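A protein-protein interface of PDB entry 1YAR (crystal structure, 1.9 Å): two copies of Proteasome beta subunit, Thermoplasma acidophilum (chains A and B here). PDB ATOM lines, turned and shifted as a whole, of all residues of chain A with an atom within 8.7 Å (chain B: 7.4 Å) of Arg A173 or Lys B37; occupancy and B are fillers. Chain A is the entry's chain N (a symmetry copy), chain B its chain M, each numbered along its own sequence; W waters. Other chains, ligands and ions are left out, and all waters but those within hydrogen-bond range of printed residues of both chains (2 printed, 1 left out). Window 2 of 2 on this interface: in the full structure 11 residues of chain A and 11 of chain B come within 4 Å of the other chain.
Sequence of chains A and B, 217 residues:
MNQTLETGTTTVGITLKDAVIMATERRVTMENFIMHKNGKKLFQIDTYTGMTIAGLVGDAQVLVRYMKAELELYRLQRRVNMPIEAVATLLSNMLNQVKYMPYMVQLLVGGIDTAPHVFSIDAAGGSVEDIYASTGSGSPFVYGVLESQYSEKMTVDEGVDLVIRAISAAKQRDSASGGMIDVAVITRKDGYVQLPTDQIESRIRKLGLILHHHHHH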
ATOM      1  N   THR A  10       6.089  -1.679  39.191  1.00  0.00           N
ATOM      2  CA  THR A  10       4.906  -1.185  39.901  1.00  0.00           C
ATOM      3  C   THR A  10       5.089  -1.363  41.407  1.00  0.00           C
ATOM      4  O   THR A  10       5.370  -2.469  41.864  1.00  0.00           O
ATOM      5  CB  THR A  10       3.642  -1.948  39.487  1.00  0.00           C
ATOM      6  OG1 THR A  10       3.526  -1.921  38.080  1.00  0.00           O
ATOM      7  CG2 THR A  10       2.388  -1.221  39.963  1.00  0.00           C
ATOM      8  N   ARG A  27       9.836  -7.549  38.210  1.00  0.00           N
ATOM      9  CA  ARG A  27      10.454  -7.597  36.905  1.00  0.00           C
ATOM     10  C   ARG A  27      11.559  -6.560  36.795  1.00  0.00           C
ATOM     11  O   ARG A  27      11.371  -5.404  37.160  1.00  0.00           O
ATOM     12  CB  ARG A  27       9.433  -7.358  35.803  1.00  0.00           C
ATOM     13  CG  ARG A  27      10.072  -7.481  34.398  1.00  0.00           C
ATOM     14  CD  ARG A  27       9.058  -7.480  33.280  1.00  0.00           C
ATOM     15  NE  ARG A  27       8.373  -8.775  33.235  1.00  0.00           N
ATOM     16  CZ  ARG A  27       7.442  -9.095  32.363  1.00  0.00           C
ATOM     17  NH1 ARG A  27       7.040  -8.206  31.468  1.00  0.00           N
ATOM     18  NH2 ARG A  27       6.888 -10.301  32.402  1.00  0.00           N
ATOM     19  N   SER A 137       6.603   2.579  36.181  1.00  0.00           N
ATOM     20  CA  SER A 137       5.860   2.625  34.919  1.00  0.00           C
ATOM     21  C   SER A 137       4.417   2.111  35.023  1.00  0.00           C
ATOM     22  O   SER A 137       3.547   2.471  34.208  1.00  0.00           O
ATOM     23  CB  SER A 137       6.611   1.813  33.858  1.00  0.00           C
ATOM     24  OG  SER A 137       7.057   0.591  34.401  1.00  0.00           O
ATOM     25  N   GLY A 138       4.184   1.242  35.999  1.00  0.00           N
ATOM     26  CA  GLY A 138       2.860   0.649  36.207  1.00  0.00           C
ATOM     27  C   GLY A 138       1.892   1.480  37.035  1.00  0.00           C
ATOM     28  O   GLY A 138       0.688   1.164  37.084  1.00  0.00           O
ATOM     29  N   PRO A 140       0.172   4.390  36.831  1.00  0.00           N
ATOM     30  CA  PRO A 140      -1.109   4.913  36.324  1.00  0.00           C
ATOM     31  C   PRO A 140      -2.239   3.887  36.392  1.00  0.00           C
ATOM     32  O   PRO A 140      -3.361   4.217  36.809  1.00  0.00           O
ATOM     33  CB  PRO A 140      -0.797   5.301  34.867  1.00  0.00           C
ATOM     34  CG  PRO A 140       0.703   5.482  34.806  1.00  0.00           C
ATOM     35  CD  PRO A 140       1.248   4.530  35.828  1.00  0.00           C
ATOM     36  N   PHE A 141      -1.938   2.637  36.051  1.00  0.00           N
ATOM     37  CA  PHE A 141      -2.914   1.552  36.118  1.00  0.00           C
ATOM     38  C   PHE A 141      -3.332   1.302  37.567  1.00  0.00           C
ATOM     39  O   PHE A 141      -4.513   1.140  37.842  1.00  0.00           O
ATOM     40  CB  PHE A 141      -2.350   0.281  35.444  1.00  0.00           C
ATOM     41  CG  PHE A 141      -1.758   0.557  34.081  1.00  0.00           C
ATOM     42  CD1 PHE A 141      -2.578   0.875  32.996  1.00  0.00           C
ATOM     43  CD2 PHE A 141      -0.372   0.559  33.898  1.00  0.00           C
ATOM     44  CE1 PHE A 141      -2.013   1.175  31.749  1.00  0.00           C
ATOM     45  CE2 PHE A 141       0.183   0.858  32.662  1.00  0.00           C
ATOM     46  CZ  PHE A 141      -0.650   1.141  31.579  1.00  0.00           C
ATOM     47  N   VAL A 142      -2.368   1.314  38.484  1.00  0.00           N
ATOM     48  CA  VAL A 142      -2.671   1.203  39.916  1.00  0.00           C
ATOM     49  C   VAL A 142      -3.568   2.354  40.363  1.00  0.00           C
ATOM     50  O   VAL A 142      -4.538   2.128  41.083  1.00  0.00           O
ATOM     51  CB  VAL A 142      -1.387   1.220  40.769  1.00  0.00           C
ATOM     52  CG1 VAL A 142      -1.711   1.248  42.272  1.00  0.00           C
ATOM     53  CG2 VAL A 142      -0.568  -0.013  40.466  1.00  0.00           C
ATOM     54  N   ALA A 166      -4.651  -4.318  42.114  1.00  0.00           N
ATOM     55  CA  ALA A 166      -4.037  -3.137  41.472  1.00  0.00           C
ATOM     56  C   ALA A 166      -2.762  -3.517  40.725  1.00  0.00           C
ATOM     57  O   ALA A 166      -2.582  -3.132  39.564  1.00  0.00           O
ATOM     58  CB  ALA A 166      -3.739  -2.076  42.505  1.00  0.00           C
ATOM     59  N   ILE A 167      -1.885  -4.274  41.382  1.00  0.00           N
ATOM     60  CA  ILE A 167      -0.634  -4.670  40.757  1.00  0.00           C
ATOM     61  C   ILE A 167      -0.883  -5.688  39.642  1.00  0.00           C
ATOM     62  O   ILE A 167      -0.225  -5.637  38.614  1.00  0.00           O
ATOM     63  CB  ILE A 167       0.360  -5.194  41.784  1.00  0.00           C
ATOM     64  CG1 ILE A 167       0.782  -4.050  42.709  1.00  0.00           C
ATOM     65  CG2 ILE A 167       1.620  -5.782  41.069  1.00  0.00           C
ATOM     66  CD1 ILE A 167       1.582  -4.521  43.889  1.00  0.00           C
ATOM     67  N   SER A 168      -1.849  -6.592  39.821  1.00  0.00           N
ATOM     68  CA  SER A 168      -2.171  -7.532  38.733  1.00  0.00           C
ATOM     69  C   SER A 168      -2.694  -6.757  37.501  1.00  0.00           C
ATOM     70  O   SER A 168      -2.334  -7.069  36.366  1.00  0.00           O
ATOM     71  CB  SER A 168      -3.198  -8.591  39.189  1.00  0.00           C
ATOM     72  OG  SER A 168      -2.761  -9.265  40.373  1.00  0.00           O
ATOM     73  N   ALA A 169      -3.534  -5.746  37.728  1.00  0.00           N
ATOM     74  CA  ALA A 169      -3.999  -4.873  36.624  1.00  0.00           C
ATOM     75  C   ALA A 169      -2.803  -4.187  35.923  1.00  0.00           C
ATOM     76  O   ALA A 169      -2.725  -4.154  34.686  1.00  0.00           O
ATOM     77  CB  ALA A 169      -5.010  -3.842  37.135  1.00  0.00           C
ATOM     78  N   ALA A 170      -1.861  -3.672  36.706  1.00  0.00           N
ATOM     79  CA  ALA A 170      -0.670  -3.050  36.136  1.00  0.00           C
ATOM     80  C   ALA A 170       0.153  -4.059  35.321  1.00  0.00           C
ATOM     81  O   ALA A 170       0.627  -3.734  34.235  1.00  0.00           O
ATOM     82  CB  ALA A 170       0.172  -2.425  37.233  1.00  0.00           C
ATOM     83  N   LYS A 171       0.305  -5.281  35.828  1.00  0.00           N
ATOM     84  CA  LYS A 171       1.051  -6.318  35.096  1.00  0.00           C
ATOM     85  C   LYS A 171       0.444  -6.613  33.737  1.00  0.00           C
ATOM     86  O   LYS A 171       1.174  -6.855  32.776  1.00  0.00           O
ATOM     87  CB  LYS A 171       1.150  -7.601  35.931  1.00  0.00           C
ATOM     88  CG  LYS A 171       2.150  -7.472  37.080  1.00  0.00           C
ATOM     89  CD  LYS A 171       2.086  -8.689  38.011  1.00  0.00           C
ATOM     90  CE  LYS A 171       2.179 -10.019  37.306  1.00  0.00           C
ATOM     91  NZ  LYS A 171       2.014 -11.095  38.354  1.00  0.00           N
ATOM     92  N   GLN A 172      -0.881  -6.532  33.641  1.00  0.00           N
ATOM     93  CA  GLN A 172      -1.584  -6.760  32.369  1.00  0.00           C
ATOM     94  C   GLN A 172      -1.311  -5.666  31.320  1.00  0.00           C
ATOM     95  O   GLN A 172      -1.418  -5.910  30.111  1.00  0.00           O
ATOM     96  CB  GLN A 172      -3.087  -6.907  32.611  1.00  0.00           C
ATOM     97  CG  GLN A 172      -3.505  -8.230  33.275  1.00  0.00           C
ATOM     98  CD  GLN A 172      -3.172  -9.451  32.429  1.00  0.00           C
ATOM     99  OE1 GLN A 172      -3.408  -9.465  31.223  1.00  0.00           O
ATOM    100  NE2 GLN A 172      -2.617 -10.468  33.058  1.00  0.00           N
ATOM    101  N   ARG A 173      -0.913  -4.472  31.769  1.00  0.00           N
ATOM    102  CA  ARG A 173      -0.847  -3.324  30.861  1.00  0.00           C
ATOM    103  C   ARG A 173       0.478  -2.595  30.781  1.00  0.00           C
ATOM    104  O   ARG A 173       0.655  -1.715  29.929  1.00  0.00           O
ATOM    105  CB  ARG A 173      -1.960  -2.332  31.226  1.00  0.00           C
ATOM    106  CG  ARG A 173      -3.349  -2.874  30.894  1.00  0.00           C
ATOM    107  CD  ARG A 173      -3.618  -2.973  29.398  1.00  0.00           C
ATOM    108  NE  ARG A 173      -4.875  -3.652  29.125  1.00  0.00           N
ATOM    109  CZ  ARG A 173      -5.360  -3.861  27.904  1.00  0.00           C
ATOM    110  NH1 ARG A 173      -4.694  -3.435  26.840  1.00  0.00           N
ATOM    111  NH2 ARG A 173      -6.515  -4.488  27.759  1.00  0.00           N
ATOM    112  N   ASP A 174       1.393  -2.941  31.670  1.00  0.00           N
ATOM    113  CA  ASP A 174       2.730  -2.351  31.671  1.00  0.00           C
ATOM    114  C   ASP A 174       3.751  -3.452  31.401  1.00  0.00           C
ATOM    115  O   ASP A 174       3.943  -4.324  32.234  1.00  0.00           O
ATOM    116  CB  ASP A 174       3.008  -1.731  33.044  1.00  0.00           C
ATOM    117  CG  ASP A 174       4.441  -1.236  33.189  1.00  0.00           C
ATOM    118  OD1 ASP A 174       5.035  -0.843  32.170  1.00  0.00           O
ATOM    119  OD2 ASP A 174       5.055  -1.208  34.273  1.00  0.00           O
ATOM    120  N   SER A 175       4.397  -3.421  30.244  1.00  0.00           N
ATOM    121  CA  SER A 175       5.355  -4.484  29.899  1.00  0.00           C
ATOM    122  C   SER A 175       6.623  -4.470  30.779  1.00  0.00           C
ATOM    123  O   SER A 175       7.350  -5.467  30.833  1.00  0.00           O
ATOM    124  CB  SER A 175       5.688  -4.454  28.396  1.00  0.00           C
ATOM    125  OG  SER A 175       6.382  -3.261  28.070  1.00  0.00           O
ATOM    126  N   ALA A 176       6.877  -3.355  31.484  1.00  0.00           N
ATOM    127  CA  ALA A 176       8.008  -3.291  32.414  1.00  0.00           C
ATOM    128  C   ALA A 176       7.673  -3.822  33.820  1.00  0.00           C
ATOM    129  O   ALA A 176       8.512  -3.801  34.741  1.00  0.00           O
ATOM    130  CB  ALA A 176       8.594  -1.865  32.473  1.00  0.00           C
ATOM    131  N   SER A 177       6.454  -4.312  33.985  1.00  0.00           N
ATOM    132  CA  SER A 177       6.034  -4.933  35.237  1.00  0.00           C
ATOM    133  C   SER A 177       5.779  -6.431  35.038  1.00  0.00           C
ATOM    134  O   SER A 177       5.393  -6.853  33.948  1.00  0.00           O
ATOM    135  CB  SER A 177       4.776  -4.237  35.768  1.00  0.00           C
ATOM    136  OG  SER A 177       5.112  -2.914  36.168  1.00  0.00           O
ATOM    137  N   GLY A 178       6.009  -7.236  36.073  1.00  0.00           N
ATOM    138  CA  GLY A 178       5.832  -8.677  35.922  1.00  0.00           C
ATOM    139  C   GLY A 178       6.326  -9.463  37.114  1.00  0.00           C
ATOM    140  O   GLY A 178       6.980  -8.917  38.001  1.00  0.00           O
ATOM    141  N   ILE A 210      -4.367 -13.996  37.582  1.00  0.00           N
ATOM    142  CA  ILE A 210      -3.299 -14.919  37.118  1.00  0.00           C
ATOM    143  C   ILE A 210      -1.911 -14.698  37.752  1.00  0.00           C
ATOM    144  O   ILE A 210      -1.629 -13.618  38.285  1.00  0.00           O
ATOM    145  CB  ILE A 210      -3.201 -15.005  35.544  1.00  0.00           C
ATOM    146  CG1 ILE A 210      -2.819 -13.653  34.921  1.00  0.00           C
ATOM    147  CG2 ILE A 210      -4.487 -15.616  34.933  1.00  0.00           C
ATOM    148  CD1 ILE A 210      -2.250 -13.771  33.504  1.00  0.00           C
ATOM    149  N   GLU B  25       3.387 -13.852  17.980  1.00  0.00           N
ATOM    150  CA  GLU B  25       2.529 -13.586  19.120  1.00  0.00           C
ATOM    151  C   GLU B  25       1.645 -12.375  18.763  1.00  0.00           C
ATOM    152  O   GLU B  25       1.481 -12.065  17.580  1.00  0.00           O
ATOM    153  CB  GLU B  25       3.346 -13.449  20.419  1.00  0.00           C
ATOM    154  CG  GLU B  25       4.616 -12.618  20.283  1.00  0.00           C
ATOM    155  CD  GLU B  25       4.322 -11.191  19.886  1.00  0.00           C
ATOM    156  OE1 GLU B  25       3.915 -10.389  20.772  1.00  0.00           O
ATOM    157  OE2 GLU B  25       4.480 -10.866  18.685  1.00  0.00           O
ATOM    158  N   ARG B  26       1.074 -11.682  19.749  1.00  0.00           N
ATOM    159  CA  ARG B  26      -0.015 -10.771  19.428  1.00  0.00           C
ATOM    160  C   ARG B  26       0.048  -9.405  20.137  1.00  0.00           C
ATOM    161  O   ARG B  26      -0.884  -8.607  20.019  1.00  0.00           O
ATOM    162  CB  ARG B  26      -1.340 -11.416  19.803  1.00  0.00           C
ATOM    163  CG  ARG B  26      -1.751 -12.685  18.998  1.00  0.00           C
ATOM    164  CD  ARG B  26      -3.158 -13.119  19.408  1.00  0.00           C
ATOM    165  NE  ARG B  26      -3.690 -14.245  18.644  1.00  0.00           N
ATOM    166  CZ  ARG B  26      -4.849 -14.857  18.915  1.00  0.00           C
ATOM    167  NH1 ARG B  26      -5.616 -14.461  19.936  1.00  0.00           N
ATOM    168  NH2 ARG B  26      -5.249 -15.874  18.159  1.00  0.00           N
ATOM    169  N   ARG B  27       1.116  -9.160  20.876  1.00  0.00           N
ATOM    170  CA  ARG B  27       1.184  -7.967  21.732  1.00  0.00           C
ATOM    171  C   ARG B  27       1.453  -6.715  20.911  1.00  0.00           C
ATOM    172  O   ARG B  27       2.370  -6.679  20.094  1.00  0.00           O
ATOM    173  CB  ARG B  27       2.282  -8.136  22.793  1.00  0.00           C
ATOM    174  CG  ARG B  27       2.420  -6.909  23.755  1.00  0.00           C
ATOM    175  CD  ARG B  27       3.278  -7.203  24.971  1.00  0.00           C
ATOM    176  NE  ARG B  27       2.598  -8.150  25.882  1.00  0.00           N
ATOM    177  CZ  ARG B  27       3.102  -8.577  27.029  1.00  0.00           C
ATOM    178  NH1 ARG B  27       4.287  -8.157  27.436  1.00  0.00           N
ATOM    179  NH2 ARG B  27       2.424  -9.426  27.782  1.00  0.00           N
ATOM    180  N   VAL B  28       0.667  -5.675  21.161  1.00  0.00           N
ATOM    181  CA  VAL B  28       0.870  -4.368  20.535  1.00  0.00           C
ATOM    182  C   VAL B  28       1.150  -3.352  21.669  1.00  0.00           C
ATOM    183  O   VAL B  28       0.302  -3.145  22.556  1.00  0.00           O
ATOM    184  CB  VAL B  28      -0.394  -3.969  19.732  1.00  0.00           C
ATOM    185  CG1 VAL B  28      -0.209  -2.633  19.031  1.00  0.00           C
ATOM    186  CG2 VAL B  28      -0.755  -5.059  18.703  1.00  0.00           C
ATOM    187  N   THR B  29       2.355  -2.797  21.666  1.00  0.00           N
ATOM    188  CA  THR B  29       2.779  -1.825  22.682  1.00  0.00           C
ATOM    189  C   THR B  29       3.023  -0.448  22.092  1.00  0.00           C
ATOM    190  O   THR B  29       3.233  -0.285  20.881  1.00  0.00           O
ATOM    191  CB  THR B  29       4.077  -2.274  23.383  1.00  0.00           C
ATOM    192  OG1 THR B  29       5.037  -2.657  22.399  1.00  0.00           O
ATOM    193  CG2 THR B  29       3.866  -3.551  24.186  1.00  0.00           C
ATOM    194  N   MET B  30       2.981   0.542  22.977  1.00  0.00           N
ATOM    195  CA  MET B  30       3.555   1.853  22.728  1.00  0.00           C
ATOM    196  C   MET B  30       4.457   2.112  23.918  1.00  0.00           C
ATOM    197  O   MET B  30       3.963   2.304  25.037  1.00  0.00           O
ATOM    198  CB  MET B  30       2.476   2.922  22.653  1.00  0.00           C
ATOM    199  CG  MET B  30       3.061   4.306  22.462  1.00  0.00           C
ATOM    200  SD  MET B  30       1.751   5.451  22.040  1.00  0.00           S
ATOM    201  CE  MET B  30       0.908   5.562  23.630  1.00  0.00           C
ATOM    202  N   ASN B  32       6.292   1.069  26.914  1.00  0.00           N
ATOM    203  CA  ASN B  32       5.936   0.012  27.893  1.00  0.00           C
ATOM    204  C   ASN B  32       4.428  -0.292  27.987  1.00  0.00           C
ATOM    205  O   ASN B  32       4.015  -1.224  28.679  1.00  0.00           O
ATOM    206  CB  ASN B  32       6.413   0.428  29.281  1.00  0.00           C
ATOM    207  CG  ASN B  32       5.704   1.695  29.770  1.00  0.00           C
ATOM    208  OD1 ASN B  32       4.823   1.641  30.664  1.00  0.00           O
ATOM    209  ND2 ASN B  32       6.041   2.840  29.150  1.00  0.00           N
ATOM    210  N   PHE B  33       3.611   0.498  27.297  1.00  0.00           N
ATOM    211  CA  PHE B  33       2.159   0.447  27.441  1.00  0.00           C
ATOM    212  C   PHE B  33       1.623  -0.654  26.520  1.00  0.00           C
ATOM    213  O   PHE B  33       1.800  -0.570  25.316  1.00  0.00           O
ATOM    214  CB  PHE B  33       1.601   1.833  27.042  1.00  0.00           C
ATOM    215  CG  PHE B  33       0.136   2.075  27.367  1.00  0.00           C
ATOM    216  CD1 PHE B  33      -0.733   1.053  27.760  1.00  0.00           C
ATOM    217  CD2 PHE B  33      -0.386   3.376  27.224  1.00  0.00           C
ATOM    218  CE1 PHE B  33      -2.106   1.310  28.007  1.00  0.00           C
ATOM    219  CE2 PHE B  33      -1.765   3.659  27.475  1.00  0.00           C
ATOM    220  CZ  PHE B  33      -2.620   2.624  27.879  1.00  0.00           C
ATOM    221  N   ILE B  34       0.979  -1.679  27.087  1.00  0.00           N
ATOM    222  CA  ILE B  34       0.358  -2.748  26.288  1.00  0.00           C
ATOM    223  C   ILE B  34      -1.047  -2.293  25.921  1.00  0.00           C
ATOM    224  O   ILE B  34      -1.965  -2.407  26.719  1.00  0.00           O
ATOM    225  CB  ILE B  34       0.305  -4.090  27.065  1.00  0.00           C
ATOM    226  CG1 ILE B  34       1.712  -4.487  27.565  1.00  0.00           C
ATOM    227  CG2 ILE B  34      -0.335  -5.196  26.174  1.00  0.00           C
ATOM    228  CD1 ILE B  34       1.718  -5.563  28.632  1.00  0.00           C
ATOM    229  N   MET B  35      -1.201  -1.756  24.719  1.00  0.00           N
ATOM    230  CA  MET B  35      -2.492  -1.241  24.267  1.00  0.00           C
ATOM    231  C   MET B  35      -3.414  -2.385  23.843  1.00  0.00           C
ATOM    232  O   MET B  35      -4.619  -2.376  24.134  1.00  0.00           O
ATOM    233  CB  MET B  35      -2.277  -0.226  23.144  1.00  0.00           C
ATOM    234  CG  MET B  35      -1.018   0.666  23.367  1.00  0.00           C
ATOM    235  SD  MET B  35      -0.864   2.201  22.405  1.00  0.00           S
ATOM    236  CE  MET B  35      -1.891   3.278  23.413  1.00  0.00           C
ATOM    237  N   HIS B  36      -2.837  -3.394  23.193  1.00  0.00           N
ATOM    238  CA  HIS B  36      -3.621  -4.501  22.691  1.00  0.00           C
ATOM    239  C   HIS B  36      -2.899  -5.793  22.945  1.00  0.00           C
ATOM    240  O   HIS B  36      -1.704  -5.907  22.674  1.00  0.00           O
ATOM    241  CB  HIS B  36      -3.871  -4.348  21.196  1.00  0.00           C
ATOM    242  CG  HIS B  36      -4.508  -3.050  20.831  1.00  0.00           C
ATOM    243  ND1 HIS B  36      -5.843  -2.791  21.060  1.00  0.00           N
ATOM    244  CD2 HIS B  36      -3.992  -1.932  20.274  1.00  0.00           C
ATOM    245  CE1 HIS B  36      -6.123  -1.567  20.644  1.00  0.00           C
ATOM    246  NE2 HIS B  36      -5.017  -1.024  20.167  1.00  0.00           N
ATOM    247  N   LYS B  37      -3.632  -6.759  23.470  1.00  0.00           N
ATOM    248  CA  LYS B  37      -3.046  -8.056  23.786  1.00  0.00           C
ATOM    249  C   LYS B  37      -3.265  -9.055  22.665  1.00  0.00           C
ATOM    250  O   LYS B  37      -2.644 -10.125  22.659  1.00  0.00           O
ATOM    251  CB  LYS B  37      -3.640  -8.632  25.065  1.00  0.00           C
ATOM    252  CG  LYS B  37      -3.663  -7.714  26.259  1.00  0.00           C
ATOM    253  CD  LYS B  37      -4.414  -8.438  27.378  1.00  0.00           C
ATOM    254  CE  LYS B  37      -4.637  -7.538  28.554  1.00  0.00           C
ATOM    255  NZ  LYS B  37      -5.390  -8.246  29.601  1.00  0.00           N
ATOM    256  N   ASN B  38      -4.145  -8.705  21.731  1.00  0.00           N
ATOM    257  CA  ASN B  38      -4.587  -9.625  20.675  1.00  0.00           C
ATOM    258  C   ASN B  38      -4.487  -9.068  19.271  1.00  0.00           C
ATOM    259  O   ASN B  38      -5.415  -9.244  18.466  1.00  0.00           O
ATOM    260  CB  ASN B  38      -6.036 -10.039  20.916  1.00  0.00           C
ATOM    261  CG  ASN B  38      -6.169 -11.092  21.982  1.00  0.00           C
ATOM    262  OD1 ASN B  38      -5.638 -12.206  21.839  1.00  0.00           O
ATOM    263  ND2 ASN B  38      -6.908 -10.769  23.061  1.00  0.00           N
ATOM    264  N   GLY B  39      -3.368  -8.414  18.964  1.00  0.00           N
ATOM    265  CA  GLY B  39      -3.110  -7.936  17.609  1.00  0.00           C
ATOM    266  C   GLY B  39      -2.956  -9.125  16.660  1.00  0.00           C
ATOM    267  O   GLY B  39      -2.720 -10.252  17.095  1.00  0.00           O
ATOM    268  N   LYS B  40      -3.127  -8.895  15.374  1.00  0.00           N
ATOM    269  CA  LYS B  40      -2.957  -9.962  14.392  1.00  0.00           C
ATOM    270  C   LYS B  40      -1.729  -9.606  13.597  1.00  0.00           C
ATOM    271  O   LYS B  40      -1.643  -8.488  13.066  1.00  0.00           O
ATOM    272  CB  LYS B  40      -4.176 -10.025  13.479  1.00  0.00           C
ATOM    273  CG  LYS B  40      -4.104 -11.122  12.426  1.00  0.00           C
ATOM    274  CD  LYS B  40      -5.420 -11.217  11.666  1.00  0.00           C
ATOM    275  CE  LYS B  40      -5.355 -12.323  10.616  1.00  0.00           C
ATOM    276  NZ  LYS B  40      -5.278 -13.613  11.310  1.00  0.00           N
ATOM    277  N   GLY B 178       4.066 -10.959  23.583  1.00  0.00           N
ATOM    278  CA  GLY B 178       3.129 -11.545  24.512  1.00  0.00           C
ATOM    279  C   GLY B 178       1.842 -11.916  23.844  1.00  0.00           C
ATOM    280  O   GLY B 178       1.659 -11.668  22.643  1.00  0.00           O
ATOM    281  N   GLY B 179       0.957 -12.529  24.623  1.00  0.00           N
ATOM    282  CA  GLY B 179      -0.362 -12.929  24.141  1.00  0.00           C
ATOM    283  C   GLY B 179      -0.351 -14.322  23.530  1.00  0.00           C
ATOM    284  O   GLY B 179       0.648 -15.042  23.572  1.00  0.00           O
ATOM    285  N   MET B 180      -1.478 -14.695  22.944  1.00  0.00           N
ATOM    286  CA  MET B 180      -1.638 -16.033  22.397  1.00  0.00           C
ATOM    287  C   MET B 180      -0.702 -16.200  21.180  1.00  0.00           C
ATOM    288  O   MET B 180      -0.485 -15.260  20.413  1.00  0.00           O
ATOM    289  CB  MET B 180      -3.105 -16.246  22.001  1.00  0.00           C
ATOM    290  CG  MET B 180      -3.390 -17.650  21.453  1.00  0.00           C
ATOM    291  SD  MET B 180      -2.942 -18.912  22.641  1.00  0.00           S
ATOM    292  CE  MET B 180      -2.877 -20.261  21.505  1.00  0.00           C
HETATM  293  O   HOH W   1       3.721   3.913  32.048  1.00  0.00           O
HETATM  294  O   HOH W   2       4.804  -9.296  30.029  1.00  0.00           O
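The backbone carbonyl oxygen (O) of Asn B32 lies within hydrogen-bond range of the backbone NH (N) of Ser A175 (2.7 Å).
The side-chain amino group (NZ) of Lys B37 is in hydrogen-bond range of the side-chain amide oxygen (OE1) of Gln A172, 2.8 Å away.
The guanidinium group of Arg A173 lies within hydrogen-bond range of the backbone carbonyl oxygen of Met B35 (2.9 Å).
The side-chain carboxylate of Asp A174 lies close to the side-chain amide oxygen of Asn B32 (2.9 Å).
The backbone carbonyl oxygen (O) of Arg A173 is in hydrogen-bond range of the backbone NH (N) of Ile B34 (2.9 Å).
The side-chain hydroxyl (OG) of Ser A177 lies within hydrogen-bond range of the side-chain carboxylate (OD2) of Asp A174, 2.6 Å away.
The guanidinium group (NH1) of Arg A27 lies within hydrogen-bond range of the backbone carbonyl oxygen (O) of Ser A175 (2.8 Å).
The side-chain carboxylate of Asp A174 sits close to the backbone NH of Ala A176, at 3.2 Å.
OG of Ser A137 sits at hydrogen-bond distance from OD2 of Asp A174, at 2.7 Å.
The backbone NH (N) of Gly A138 lies within hydrogen-bond range of the side-chain carboxylate (OD2) of Asp A174, 3.1 Å away.
O of Val B28 is in hydrogen-bond range of N of Met B35, 3.0 Å away.
CB of Ser A137 touches OD1 of Asn B32, 3.7 Å away.
CE1 of Phe A141 touches CE1 of Phe B33, at 3.7 Å.
O of Gln A172 touches CD1 of Ile B34, at 3.5 Å.
Asn B32 touches Arg A173 (O to O, 3.6 Å).
O of Arg A173 touches CA of Phe B33, at 3.6 Å.
Lys B37 touches Arg A173.
N of Ser A175 touches CD1 of Ile B34, at 3.8 Å.
Of chain B, only Asn B32 (3.6 Å), Phe B33 (3.6 Å), Ile B34 (2.9 Å), Met B35 (2.9 Å) and Lys B37 (3.7 Å) come within 4 Å of Arg A173.
Of the printed residues of chain A, Lys B37 touches Gln A172 and Arg A173.
Ile B34 touches just these residues of chain A: Gln A172 (3.5 Å), Arg A173 (2.9 Å) and Ser A175 (3.8 Å).
Of the printed residues of chain A, Asn B32 touches Ser A137, Arg A173, Asp A174 and Ser A175.
Of the printed residues of chain B, Ser A137 touches Asn B32 (3.7 Å).
Printed residues of chain B within 4 Å of Ser A175: Asn B32 (2.7 Å) and Ile B34 (3.8 Å).
Val A142 touches none of the printed residues of chain B.
Ile A167 touches none of the printed residues of chain B.
The nearest printed residue of chain A that does not touch Met B35 is Gln A172 (6.8 Å).
Of the 18 printed residues of chain B, 5 touch a printed residue of chain A.
Hydrophobic or aromatic side chains of chain B within 4 Å of the printed part of chain A: Phe B33 and Ile B34.
Of the 21 printed residues of chain A, 6 touch a printed residue of chain B.
Hydrophobic or aromatic side chains of chain A within 4 Å of the printed part of chain B: Phe A141.
Among the printed residues, no Asp or Glu carboxylate lies within 4 Å of a Lys or Arg side-chain nitrogen of the other chain.
2 positions are printed for both chains.
Water W1 bridges the backbone carbonyl oxygen (O) of Ser A137 (2.6 Å) and the side-chain amide oxygen (OD1) of Asn B32 (2.9 Å).
Water W2 bridges the guanidinium group of Arg A27 (2.9 Å) and the guanidinium group of Arg B27 (2.9 Å).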
